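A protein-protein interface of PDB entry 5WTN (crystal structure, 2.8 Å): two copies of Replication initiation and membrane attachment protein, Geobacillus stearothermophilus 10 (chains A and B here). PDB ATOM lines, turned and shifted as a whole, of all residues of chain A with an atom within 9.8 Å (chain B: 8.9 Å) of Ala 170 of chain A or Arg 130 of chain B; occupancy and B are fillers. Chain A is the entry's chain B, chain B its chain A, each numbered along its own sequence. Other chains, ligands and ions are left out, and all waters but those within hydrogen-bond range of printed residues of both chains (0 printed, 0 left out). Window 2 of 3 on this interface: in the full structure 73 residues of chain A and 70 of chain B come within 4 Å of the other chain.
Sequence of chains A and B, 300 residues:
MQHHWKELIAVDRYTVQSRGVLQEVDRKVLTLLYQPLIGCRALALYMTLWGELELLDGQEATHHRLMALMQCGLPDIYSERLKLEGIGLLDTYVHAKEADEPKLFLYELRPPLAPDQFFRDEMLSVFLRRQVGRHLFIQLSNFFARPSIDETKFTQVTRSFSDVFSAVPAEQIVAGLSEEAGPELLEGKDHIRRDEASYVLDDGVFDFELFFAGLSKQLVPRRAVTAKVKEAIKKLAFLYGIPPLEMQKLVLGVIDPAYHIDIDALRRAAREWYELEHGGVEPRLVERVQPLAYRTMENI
N of Arg 284 of chain A sits at hydrogen-bond distance from O of Val 168 of chain A, 2.7 Å away.
Arg 130 of chain B touches Ala 170 of chain A.
CB of Leu 239 of chain A touches CG of Met 123 of chain B (3.4 Å).
CG2 of Val 126 of chain B touches CD1 of Leu 239 of chain A (3.3 Å).
CD1 of Leu 239 of chain A touches CE1 of Phe 127 of chain B, 3.9 Å away.
OE2 of Glu 282 of chain A touches CD of Arg 129 of chain B, at 3.8 Å.
Glu 282 of chain A touches Arg 130 of chain B (OE1 to CD, 3.9 Å).
Val 126 of chain B touches Pro 283 of chain A (CG2 to CD, 3.97 Å).
Arg 130 of chain B touches Pro 283 of chain A.
Phe 127 of chain B touches Arg 284 of chain A.
N of Leu 285 of chain A touches CD1 of Phe 127 of chain B, at 3.6 Å.
Of chain B, only Arg 130 (3.5 Å) comes within 4 Å of Ala 170 of chain A.
Arg 130 of chain B touches just these residues of chain A: Ala 170 (3.5 Å), Glu 282 (3.9 Å) and Pro 283 (3.2 Å).
Pro 169 of chain A touches none of the printed residues of chain B.
Of the printed residues of chain A, Val 126 of chain B touches Leu 239 (3.3 Å) and Pro 283 (3.97 Å).
Of the printed residues of chain B, Arg 284 of chain A touches Phe 127 (3.8 Å).
Of the printed residues of chain A, Arg 129 of chain B touches Glu 282.
Gly 133 of chain B touches none of the printed residues of chain A.
Glu 171 of chain A touches none of the printed residues of chain B.
The nearest printed residue of chain B that does not touch Ala 170 of chain A is Gln 131 of chain B (8.9 Å).
The nearest printed residue of chain A that does not touch Arg 129 of chain B is Tyr 240 of chain A (5.7 Å).
Hydrophobic or aromatic side chains of chain B within 4 Å of the printed part of chain A: Met 123, Val 126 and Phe 127.
Of the 17 printed residues of chain A, 6 touch a printed residue of chain B.
Printed residues of chain A that touch a printed residue of chain B: Ala 170, Leu 239, Glu 282, Pro 283, Arg 284 and Leu 285.
Hydrophobic or aromatic side chains of chain A within 4 Å of the printed part of chain B: Ala 170, Leu 239, Pro 283 and Leu 285.
No position is printed for both chains.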
ATOM      1  N   ALA A 167      18.878  13.595  19.580  1.00  0.00           N
ATOM      2  CA  ALA A 167      19.614  14.826  19.841  1.00  0.00           C
ATOM      3  C   ALA A 167      20.613  15.126  18.726  1.00  0.00           C
ATOM      4  O   ALA A 167      21.391  14.259  18.326  1.00  0.00           O
ATOM      5  CB  ALA A 167      20.340  14.728  21.161  1.00  0.00           C
ATOM      6  N   VAL A 168      20.606  16.357  18.233  1.00  0.00           N
ATOM      7  CA  VAL A 168      21.534  16.751  17.182  1.00  0.00           C
ATOM      8  C   VAL A 168      21.943  18.199  17.407  1.00  0.00           C
ATOM      9  O   VAL A 168      21.161  18.982  17.945  1.00  0.00           O
ATOM     10  CB  VAL A 168      20.891  16.622  15.791  1.00  0.00           C
ATOM     11  CG1 VAL A 168      20.667  15.160  15.417  1.00  0.00           C
ATOM     12  CG2 VAL A 168      19.580  17.360  15.770  1.00  0.00           C
ATOM     13  N   PRO A 169      23.185  18.555  17.030  1.00  0.00           N
ATOM     14  CA  PRO A 169      23.707  19.934  17.071  1.00  0.00           C
ATOM     15  C   PRO A 169      23.126  20.815  15.954  1.00  0.00           C
ATOM     16  O   PRO A 169      22.859  20.282  14.877  1.00  0.00           O
ATOM     17  CB  PRO A 169      25.207  19.737  16.836  1.00  0.00           C
ATOM     18  CG  PRO A 169      25.471  18.309  17.207  1.00  0.00           C
ATOM     19  CD  PRO A 169      24.253  17.569  16.790  1.00  0.00           C
ATOM     20  N   ALA A 170      22.961  22.118  16.176  1.00  0.00           N
ATOM     21  CA  ALA A 170      22.408  22.998  15.137  1.00  0.00           C
ATOM     22  C   ALA A 170      23.140  24.341  15.018  1.00  0.00           C
ATOM     23  O   ALA A 170      23.950  24.688  15.878  1.00  0.00           O
ATOM     24  CB  ALA A 170      20.921  23.222  15.373  1.00  0.00           C
ATOM     25  N   GLU A 171      22.851  25.094  13.955  1.00  0.00           N
ATOM     26  CA  GLU A 171      23.479  26.406  13.766  1.00  0.00           C
ATOM     27  C   GLU A 171      23.008  27.439  14.795  1.00  0.00           C
ATOM     28  O   GLU A 171      23.769  27.843  15.678  1.00  0.00           O
ATOM     29  CB  GLU A 171      23.269  26.927  12.332  1.00  0.00           C
ATOM     30  CG  GLU A 171      23.611  28.420  12.119  1.00  0.00           C
ATOM     31  CD  GLU A 171      25.099  28.749  12.287  1.00  0.00           C
ATOM     32  OE1 GLU A 171      25.440  29.954  12.307  1.00  0.00           O
ATOM     33  OE2 GLU A 171      25.927  27.817  12.393  1.00  0.00           O
ATOM     34  N   LEU A 239      21.700  13.412  25.572  1.00  0.00           N
ATOM     35  CA  LEU A 239      21.465  14.810  25.215  1.00  0.00           C
ATOM     36  C   LEU A 239      22.653  15.436  24.493  1.00  0.00           C
ATOM     37  O   LEU A 239      22.489  16.199  23.542  1.00  0.00           O
ATOM     38  CB  LEU A 239      21.119  15.628  26.461  1.00  0.00           C
ATOM     39  CG  LEU A 239      21.360  17.136  26.370  1.00  0.00           C
ATOM     40  CD1 LEU A 239      20.214  17.821  25.640  1.00  0.00           C
ATOM     41  CD2 LEU A 239      21.553  17.736  27.754  1.00  0.00           C
ATOM     42  N   TYR A 240      23.849  15.103  24.961  1.00  0.00           N
ATOM     43  CA  TYR A 240      25.085  15.645  24.422  1.00  0.00           C
ATOM     44  C   TYR A 240      25.896  14.668  23.564  1.00  0.00           C
ATOM     45  O   TYR A 240      27.011  14.994  23.146  1.00  0.00           O
ATOM     46  CB  TYR A 240      25.931  16.194  25.572  1.00  0.00           C
ATOM     47  CG  TYR A 240      25.358  17.441  26.208  1.00  0.00           C
ATOM     48  CD1 TYR A 240      24.886  18.486  25.433  1.00  0.00           C
ATOM     49  CD2 TYR A 240      25.287  17.574  27.585  1.00  0.00           C
ATOM     50  CE1 TYR A 240      24.379  19.639  26.016  1.00  0.00           C
ATOM     51  CE2 TYR A 240      24.776  18.729  28.174  1.00  0.00           C
ATOM     52  CZ  TYR A 240      24.326  19.751  27.380  1.00  0.00           C
ATOM     53  OH  TYR A 240      23.812  20.896  27.937  1.00  0.00           O
ATOM     54  N   TYR A 274      30.464  19.603  25.736  1.00  0.00           N
ATOM     55  CA  TYR A 274      29.733  19.630  24.470  1.00  0.00           C
ATOM     56  C   TYR A 274      30.105  20.895  23.723  1.00  0.00           C
ATOM     57  O   TYR A 274      30.262  20.882  22.498  1.00  0.00           O
ATOM     58  CB  TYR A 274      28.222  19.584  24.717  1.00  0.00           C
ATOM     59  CG  TYR A 274      27.331  19.522  23.479  1.00  0.00           C
ATOM     60  CD1 TYR A 274      26.744  20.670  22.959  1.00  0.00           C
ATOM     61  CD2 TYR A 274      27.031  18.309  22.869  1.00  0.00           C
ATOM     62  CE1 TYR A 274      25.910  20.615  21.854  1.00  0.00           C
ATOM     63  CE2 TYR A 274      26.200  18.246  21.767  1.00  0.00           C
ATOM     64  CZ  TYR A 274      25.645  19.402  21.268  1.00  0.00           C
ATOM     65  OH  TYR A 274      24.817  19.339  20.177  1.00  0.00           O
ATOM     66  N   HIS A 278      31.649  20.793  20.014  1.00  0.00           N
ATOM     67  CA  HIS A 278      30.900  21.326  18.872  1.00  0.00           C
ATOM     68  C   HIS A 278      30.931  22.851  18.694  1.00  0.00           C
ATOM     69  O   HIS A 278      30.348  23.376  17.741  1.00  0.00           O
ATOM     70  CB  HIS A 278      29.464  20.796  18.865  1.00  0.00           C
ATOM     71  CG  HIS A 278      29.377  19.303  18.786  1.00  0.00           C
ATOM     72  ND1 HIS A 278      30.490  18.493  18.694  1.00  0.00           N
ATOM     73  CD2 HIS A 278      28.309  18.471  18.791  1.00  0.00           C
ATOM     74  CE1 HIS A 278      30.111  17.228  18.645  1.00  0.00           C
ATOM     75  NE2 HIS A 278      28.791  17.187  18.701  1.00  0.00           N
ATOM     76  N   GLY A 279      31.609  23.555  19.597  1.00  0.00           N
ATOM     77  CA  GLY A 279      31.704  25.002  19.516  1.00  0.00           C
ATOM     78  C   GLY A 279      30.504  25.809  19.982  1.00  0.00           C
ATOM     79  O   GLY A 279      30.065  26.708  19.269  1.00  0.00           O
ATOM     80  N   GLY A 280      29.978  25.500  21.169  1.00  0.00           N
ATOM     81  CA  GLY A 280      28.898  26.278  21.771  1.00  0.00           C
ATOM     82  C   GLY A 280      27.609  26.275  20.964  1.00  0.00           C
ATOM     83  O   GLY A 280      26.880  27.267  20.898  1.00  0.00           O
ATOM     84  N   VAL A 281      27.284  25.144  20.343  1.00  0.00           N
ATOM     85  CA  VAL A 281      26.148  25.087  19.410  1.00  0.00           C
ATOM     86  C   VAL A 281      24.758  24.802  20.007  1.00  0.00           C
ATOM     87  O   VAL A 281      23.738  25.183  19.429  1.00  0.00           O
ATOM     88  CB  VAL A 281      26.409  24.069  18.281  1.00  0.00           C
ATOM     89  CG1 VAL A 281      27.507  24.573  17.356  1.00  0.00           C
ATOM     90  CG2 VAL A 281      26.775  22.712  18.863  1.00  0.00           C
ATOM     91  N   GLU A 282      24.726  24.129  21.150  1.00  0.00           N
ATOM     92  CA  GLU A 282      23.476  23.644  21.796  1.00  0.00           C
ATOM     93  C   GLU A 282      22.779  22.498  21.049  1.00  0.00           C
ATOM     94  O   GLU A 282      22.762  22.462  19.820  1.00  0.00           O
ATOM     95  CB  GLU A 282      22.453  24.769  21.969  1.00  0.00           C
ATOM     96  CG  GLU A 282      22.459  25.504  23.283  1.00  0.00           C
ATOM     97  CD  GLU A 282      21.386  26.595  23.310  1.00  0.00           C
ATOM     98  OE1 GLU A 282      21.090  27.171  22.235  1.00  0.00           O
ATOM     99  OE2 GLU A 282      20.824  26.867  24.397  1.00  0.00           O
ATOM    100  N   PRO A 283      22.155  21.578  21.800  1.00  0.00           N
ATOM    101  CA  PRO A 283      21.420  20.456  21.201  1.00  0.00           C
ATOM    102  C   PRO A 283      20.006  20.832  20.756  1.00  0.00           C
ATOM    103  O   PRO A 283      19.372  21.685  21.392  1.00  0.00           O
ATOM    104  CB  PRO A 283      21.348  19.430  22.340  1.00  0.00           C
ATOM    105  CG  PRO A 283      22.368  19.857  23.323  1.00  0.00           C
ATOM    106  CD  PRO A 283      22.426  21.348  23.227  1.00  0.00           C
ATOM    107  N   ARG A 284      19.511  20.165  19.715  1.00  0.00           N
ATOM    108  CA  ARG A 284      18.157  20.378  19.232  1.00  0.00           C
ATOM    109  C   ARG A 284      17.408  19.057  19.311  1.00  0.00           C
ATOM    110  O   ARG A 284      17.999  17.997  19.088  1.00  0.00           O
ATOM    111  CB  ARG A 284      18.190  20.901  17.785  1.00  0.00           C
ATOM    112  CG  ARG A 284      16.816  21.191  17.152  1.00  0.00           C
ATOM    113  CD  ARG A 284      16.921  22.111  15.926  1.00  0.00           C
ATOM    114  NE  ARG A 284      16.113  21.613  14.811  1.00  0.00           N
ATOM    115  CZ  ARG A 284      16.606  20.942  13.772  1.00  0.00           C
ATOM    116  NH1 ARG A 284      17.913  20.704  13.693  1.00  0.00           N
ATOM    117  NH2 ARG A 284      15.795  20.514  12.806  1.00  0.00           N
ATOM    118  N   LEU A 285      16.122  19.101  19.646  1.00  0.00           N
ATOM    119  CA  LEU A 285      15.323  17.875  19.657  1.00  0.00           C
ATOM    120  C   LEU A 285      14.681  17.684  18.289  1.00  0.00           C
ATOM    121  O   LEU A 285      14.122  18.635  17.724  1.00  0.00           O
ATOM    122  CB  LEU A 285      14.244  17.928  20.734  1.00  0.00           C
ATOM    123  CG  LEU A 285      13.440  16.648  20.967  1.00  0.00           C
ATOM    124  CD1 LEU A 285      14.357  15.555  21.460  1.00  0.00           C
ATOM    125  CD2 LEU A 285      12.299  16.891  21.962  1.00  0.00           C
ATOM    126  N   VAL A 286      14.785  16.462  17.758  1.00  0.00           N
ATOM    127  CA  VAL A 286      14.307  16.129  16.416  1.00  0.00           C
ATOM    128  C   VAL A 286      13.729  14.711  16.341  1.00  0.00           C
ATOM    129  O   VAL A 286      14.046  13.859  17.187  1.00  0.00           O
ATOM    130  CB  VAL A 286      15.439  16.220  15.368  1.00  0.00           C
ATOM    131  CG1 VAL A 286      15.980  17.629  15.268  1.00  0.00           C
ATOM    132  CG2 VAL A 286      16.554  15.212  15.682  1.00  0.00           C
ATOM    133  N   PRO B  36       6.493  23.680  22.509  1.00  0.00           N
ATOM    134  CA  PRO B  36       7.682  23.923  21.675  1.00  0.00           C
ATOM    135  C   PRO B  36       8.484  22.652  21.356  1.00  0.00           C
ATOM    136  O   PRO B  36       9.093  22.563  20.292  1.00  0.00           O
ATOM    137  CB  PRO B  36       8.509  24.871  22.528  1.00  0.00           C
ATOM    138  CG  PRO B  36       7.485  25.643  23.279  1.00  0.00           C
ATOM    139  CD  PRO B  36       6.411  24.643  23.624  1.00  0.00           C
ATOM    140  N   LEU B  37       8.480  21.674  22.252  1.00  0.00           N
ATOM    141  CA  LEU B  37       9.202  20.454  21.984  1.00  0.00           C
ATOM    142  C   LEU B  37       8.453  19.506  21.033  1.00  0.00           C
ATOM    143  O   LEU B  37       9.049  18.994  20.088  1.00  0.00           O
ATOM    144  CB  LEU B  37       9.587  19.762  23.292  1.00  0.00           C
ATOM    145  CG  LEU B  37      10.527  20.553  24.228  1.00  0.00           C
ATOM    146  CD1 LEU B  37      11.120  19.651  25.310  1.00  0.00           C
ATOM    147  CD2 LEU B  37      11.627  21.259  23.465  1.00  0.00           C
ATOM    148  N   MET B 123      17.360  16.792  30.375  1.00  0.00           N
ATOM    149  CA  MET B 123      17.125  16.942  28.944  1.00  0.00           C
ATOM    150  C   MET B 123      16.128  18.031  28.517  1.00  0.00           C
ATOM    151  O   MET B 123      16.420  18.829  27.642  1.00  0.00           O
ATOM    152  CB  MET B 123      16.790  15.570  28.338  1.00  0.00           C
ATOM    153  CG  MET B 123      17.986  14.929  27.706  1.00  0.00           C
ATOM    154  SD  MET B 123      17.727  13.251  27.241  1.00  0.00           S
ATOM    155  CE  MET B 123      16.005  13.253  26.803  1.00  0.00           C
ATOM    156  N   LEU B 124      14.973  18.080  29.171  1.00  0.00           N
ATOM    157  CA  LEU B 124      13.866  18.905  28.706  1.00  0.00           C
ATOM    158  C   LEU B 124      14.179  20.380  28.746  1.00  0.00           C
ATOM    159  O   LEU B 124      13.860  21.096  27.816  1.00  0.00           O
ATOM    160  CB  LEU B 124      12.600  18.605  29.505  1.00  0.00           C
ATOM    161  CG  LEU B 124      12.105  17.177  29.294  1.00  0.00           C
ATOM    162  CD1 LEU B 124      10.872  16.853  30.134  1.00  0.00           C
ATOM    163  CD2 LEU B 124      11.822  16.978  27.821  1.00  0.00           C
ATOM    164  N   SER B 125      14.803  20.830  29.826  1.00  0.00           N
ATOM    165  CA  SER B 125      15.201  22.221  29.949  1.00  0.00           C
ATOM    166  C   SER B 125      16.158  22.638  28.837  1.00  0.00           C
ATOM    167  O   SER B 125      15.934  23.660  28.203  1.00  0.00           O
ATOM    168  CB  SER B 125      15.841  22.457  31.308  1.00  0.00           C
ATOM    169  OG  SER B 125      16.782  21.429  31.554  1.00  0.00           O
ATOM    170  N   VAL B 126      17.215  21.873  28.570  1.00  0.00           N
ATOM    171  CA  VAL B 126      18.129  22.352  27.530  1.00  0.00           C
ATOM    172  C   VAL B 126      17.498  22.320  26.128  1.00  0.00           C
ATOM    173  O   VAL B 126      17.635  23.279  25.371  1.00  0.00           O
ATOM    174  CB  VAL B 126      19.639  21.858  27.632  1.00  0.00           C
ATOM    175  CG1 VAL B 126      19.917  21.131  28.922  1.00  0.00           C
ATOM    176  CG2 VAL B 126      20.067  21.068  26.412  1.00  0.00           C
ATOM    177  N   PHE B 127      16.762  21.265  25.804  1.00  0.00           N
ATOM    178  CA  PHE B 127      15.944  21.296  24.596  1.00  0.00           C
ATOM    179  C   PHE B 127      15.052  22.528  24.500  1.00  0.00           C
ATOM    180  O   PHE B 127      15.017  23.193  23.471  1.00  0.00           O
ATOM    181  CB  PHE B 127      15.076  20.065  24.502  1.00  0.00           C
ATOM    182  CG  PHE B 127      15.824  18.835  24.137  1.00  0.00           C
ATOM    183  CD1 PHE B 127      16.807  18.869  23.169  1.00  0.00           C
ATOM    184  CD2 PHE B 127      15.553  17.633  24.775  1.00  0.00           C
ATOM    185  CE1 PHE B 127      17.495  17.735  22.833  1.00  0.00           C
ATOM    186  CE2 PHE B 127      16.245  16.493  24.449  1.00  0.00           C
ATOM    187  CZ  PHE B 127      17.214  16.542  23.478  1.00  0.00           C
ATOM    188  N   LEU B 128      14.323  22.836  25.563  1.00  0.00           N
ATOM    189  CA  LEU B 128      13.406  23.959  25.506  1.00  0.00           C
ATOM    190  C   LEU B 128      14.119  25.297  25.250  1.00  0.00           C
ATOM    191  O   LEU B 128      13.645  26.111  24.449  1.00  0.00           O
ATOM    192  CB  LEU B 128      12.524  24.014  26.754  1.00  0.00           C
ATOM    193  CG  LEU B 128      11.484  25.134  26.669  1.00  0.00           C
ATOM    194  CD1 LEU B 128      10.442  24.846  25.622  1.00  0.00           C
ATOM    195  CD2 LEU B 128      10.827  25.390  27.980  1.00  0.00           C
ATOM    196  N   ARG B 129      15.254  25.516  25.919  1.00  0.00           N
ATOM    197  CA  ARG B 129      16.048  26.733  25.723  1.00  0.00           C
ATOM    198  C   ARG B 129      16.379  26.949  24.250  1.00  0.00           C
ATOM    199  O   ARG B 129      16.150  28.034  23.711  1.00  0.00           O
ATOM    200  CB  ARG B 129      17.345  26.682  26.546  1.00  0.00           C
ATOM    201  CG  ARG B 129      17.953  28.045  26.880  1.00  0.00           C
ATOM    202  CD  ARG B 129      19.204  27.910  27.730  1.00  0.00           C
ATOM    203  NE  ARG B 129      18.992  27.056  28.899  1.00  0.00           N
ATOM    204  CZ  ARG B 129      19.762  26.010  29.236  1.00  0.00           C
ATOM    205  NH1 ARG B 129      20.830  25.694  28.496  1.00  0.00           N
ATOM    206  NH2 ARG B 129      19.474  25.275  30.321  1.00  0.00           N
ATOM    207  N   ARG B 130      16.902  25.903  23.608  1.00  0.00           N
ATOM    208  CA  ARG B 130      17.313  25.948  22.206  1.00  0.00           C
ATOM    209  C   ARG B 130      16.159  26.267  21.289  1.00  0.00           C
ATOM    210  O   ARG B 130      16.300  27.025  20.351  1.00  0.00           O
ATOM    211  CB  ARG B 130      17.950  24.617  21.780  1.00  0.00           C
ATOM    212  CG  ARG B 130      18.020  24.380  20.260  1.00  0.00           C
ATOM    213  CD  ARG B 130      18.924  25.394  19.563  1.00  0.00           C
ATOM    214  NE  ARG B 130      18.738  25.425  18.109  1.00  0.00           N
ATOM    215  CZ  ARG B 130      19.414  26.232  17.295  1.00  0.00           C
ATOM    216  NH1 ARG B 130      20.315  27.067  17.798  1.00  0.00           N
ATOM    217  NH2 ARG B 130      19.196  26.205  15.985  1.00  0.00           N
ATOM    218  N   GLN B 131      15.011  25.645  21.541  1.00  0.00           N
ATOM    219  CA  GLN B 131      13.872  25.738  20.627  1.00  0.00           C
ATOM    220  C   GLN B 131      13.036  27.004  20.805  1.00  0.00           C
ATOM    221  O   GLN B 131      12.257  27.372  19.925  1.00  0.00           O
ATOM    222  CB  GLN B 131      12.979  24.502  20.765  1.00  0.00           C
ATOM    223  CG  GLN B 131      11.579  24.680  20.199  1.00  0.00           C
ATOM    224  CD  GLN B 131      11.528  24.476  18.697  1.00  0.00           C
ATOM    225  OE1 GLN B 131      10.687  25.054  18.009  1.00  0.00           O
ATOM    226  NE2 GLN B 131      12.432  23.649  18.181  1.00  0.00           N
ATOM    227  N   VAL B 132      13.198  27.661  21.946  1.00  0.00           N
ATOM    228  CA  VAL B 132      12.434  28.846  22.267  1.00  0.00           C
ATOM    229  C   VAL B 132      13.271  30.119  22.377  1.00  0.00           C
ATOM    230  O   VAL B 132      12.746  31.237  22.315  1.00  0.00           O
ATOM    231  CB  VAL B 132      11.669  28.564  23.575  1.00  0.00           C
ATOM    232  CG1 VAL B 132      12.035  29.542  24.683  1.00  0.00           C
ATOM    233  CG2 VAL B 132      10.172  28.486  23.312  1.00  0.00           C
ATOM    234  N   GLY B 133      14.586  29.947  22.482  1.00  0.00           N
ATOM    235  CA  GLY B 133      15.475  31.074  22.685  1.00  0.00           C
ATOM    236  C   GLY B 133      15.620  31.552  24.121  1.00  0.00           C
ATOM    237  O   GLY B 133      14.695  31.442  24.916  1.00  0.00           O
ATOM    238  N   ARG B 134      16.770  32.146  24.429  1.00  0.00           N
ATOM    239  CA  ARG B 134      17.135  32.510  25.803  1.00  0.00           C
ATOM    240  C   ARG B 134      16.173  33.478  26.500  1.00  0.00           C
ATOM    241  O   ARG B 134      15.797  33.270  27.650  1.00  0.00           O
ATOM    242  CB  ARG B 134      18.551  33.086  25.841  1.00  0.00           C
ATOM    243  CG  ARG B 134      19.118  33.273  27.248  1.00  0.00           C
ATOM    244  CD  ARG B 134      19.767  31.987  27.777  1.00  0.00           C
ATOM    245  NE  ARG B 134      20.780  31.445  26.856  1.00  0.00           N
ATOM    246  CZ  ARG B 134      21.625  30.446  27.135  1.00  0.00           C
ATOM    247  NH1 ARG B 134      21.614  29.858  28.330  1.00  0.00           N
ATOM    248  NH2 ARG B 134      22.497  30.038  26.213  1.00  0.00           N
ATOM    249  N   PHE B 137      12.821  31.781  27.189  1.00  0.00           N
ATOM    250  CA  PHE B 137      13.042  30.755  28.184  1.00  0.00           C
ATOM    251  C   PHE B 137      12.954  31.327  29.589  1.00  0.00           C
ATOM    252  O   PHE B 137      12.366  30.712  30.468  1.00  0.00           O
ATOM    253  CB  PHE B 137      14.407  30.109  27.972  1.00  0.00           C
ATOM    254  CG  PHE B 137      14.679  28.944  28.887  1.00  0.00           C
ATOM    255  CD1 PHE B 137      14.101  27.702  28.657  1.00  0.00           C
ATOM    256  CD2 PHE B 137      15.532  29.081  29.962  1.00  0.00           C
ATOM    257  CE1 PHE B 137      14.366  26.642  29.494  1.00  0.00           C
ATOM    258  CE2 PHE B 137      15.801  28.022  30.799  1.00  0.00           C
ATOM    259  CZ  PHE B 137      15.225  26.810  30.572  1.00  0.00           C
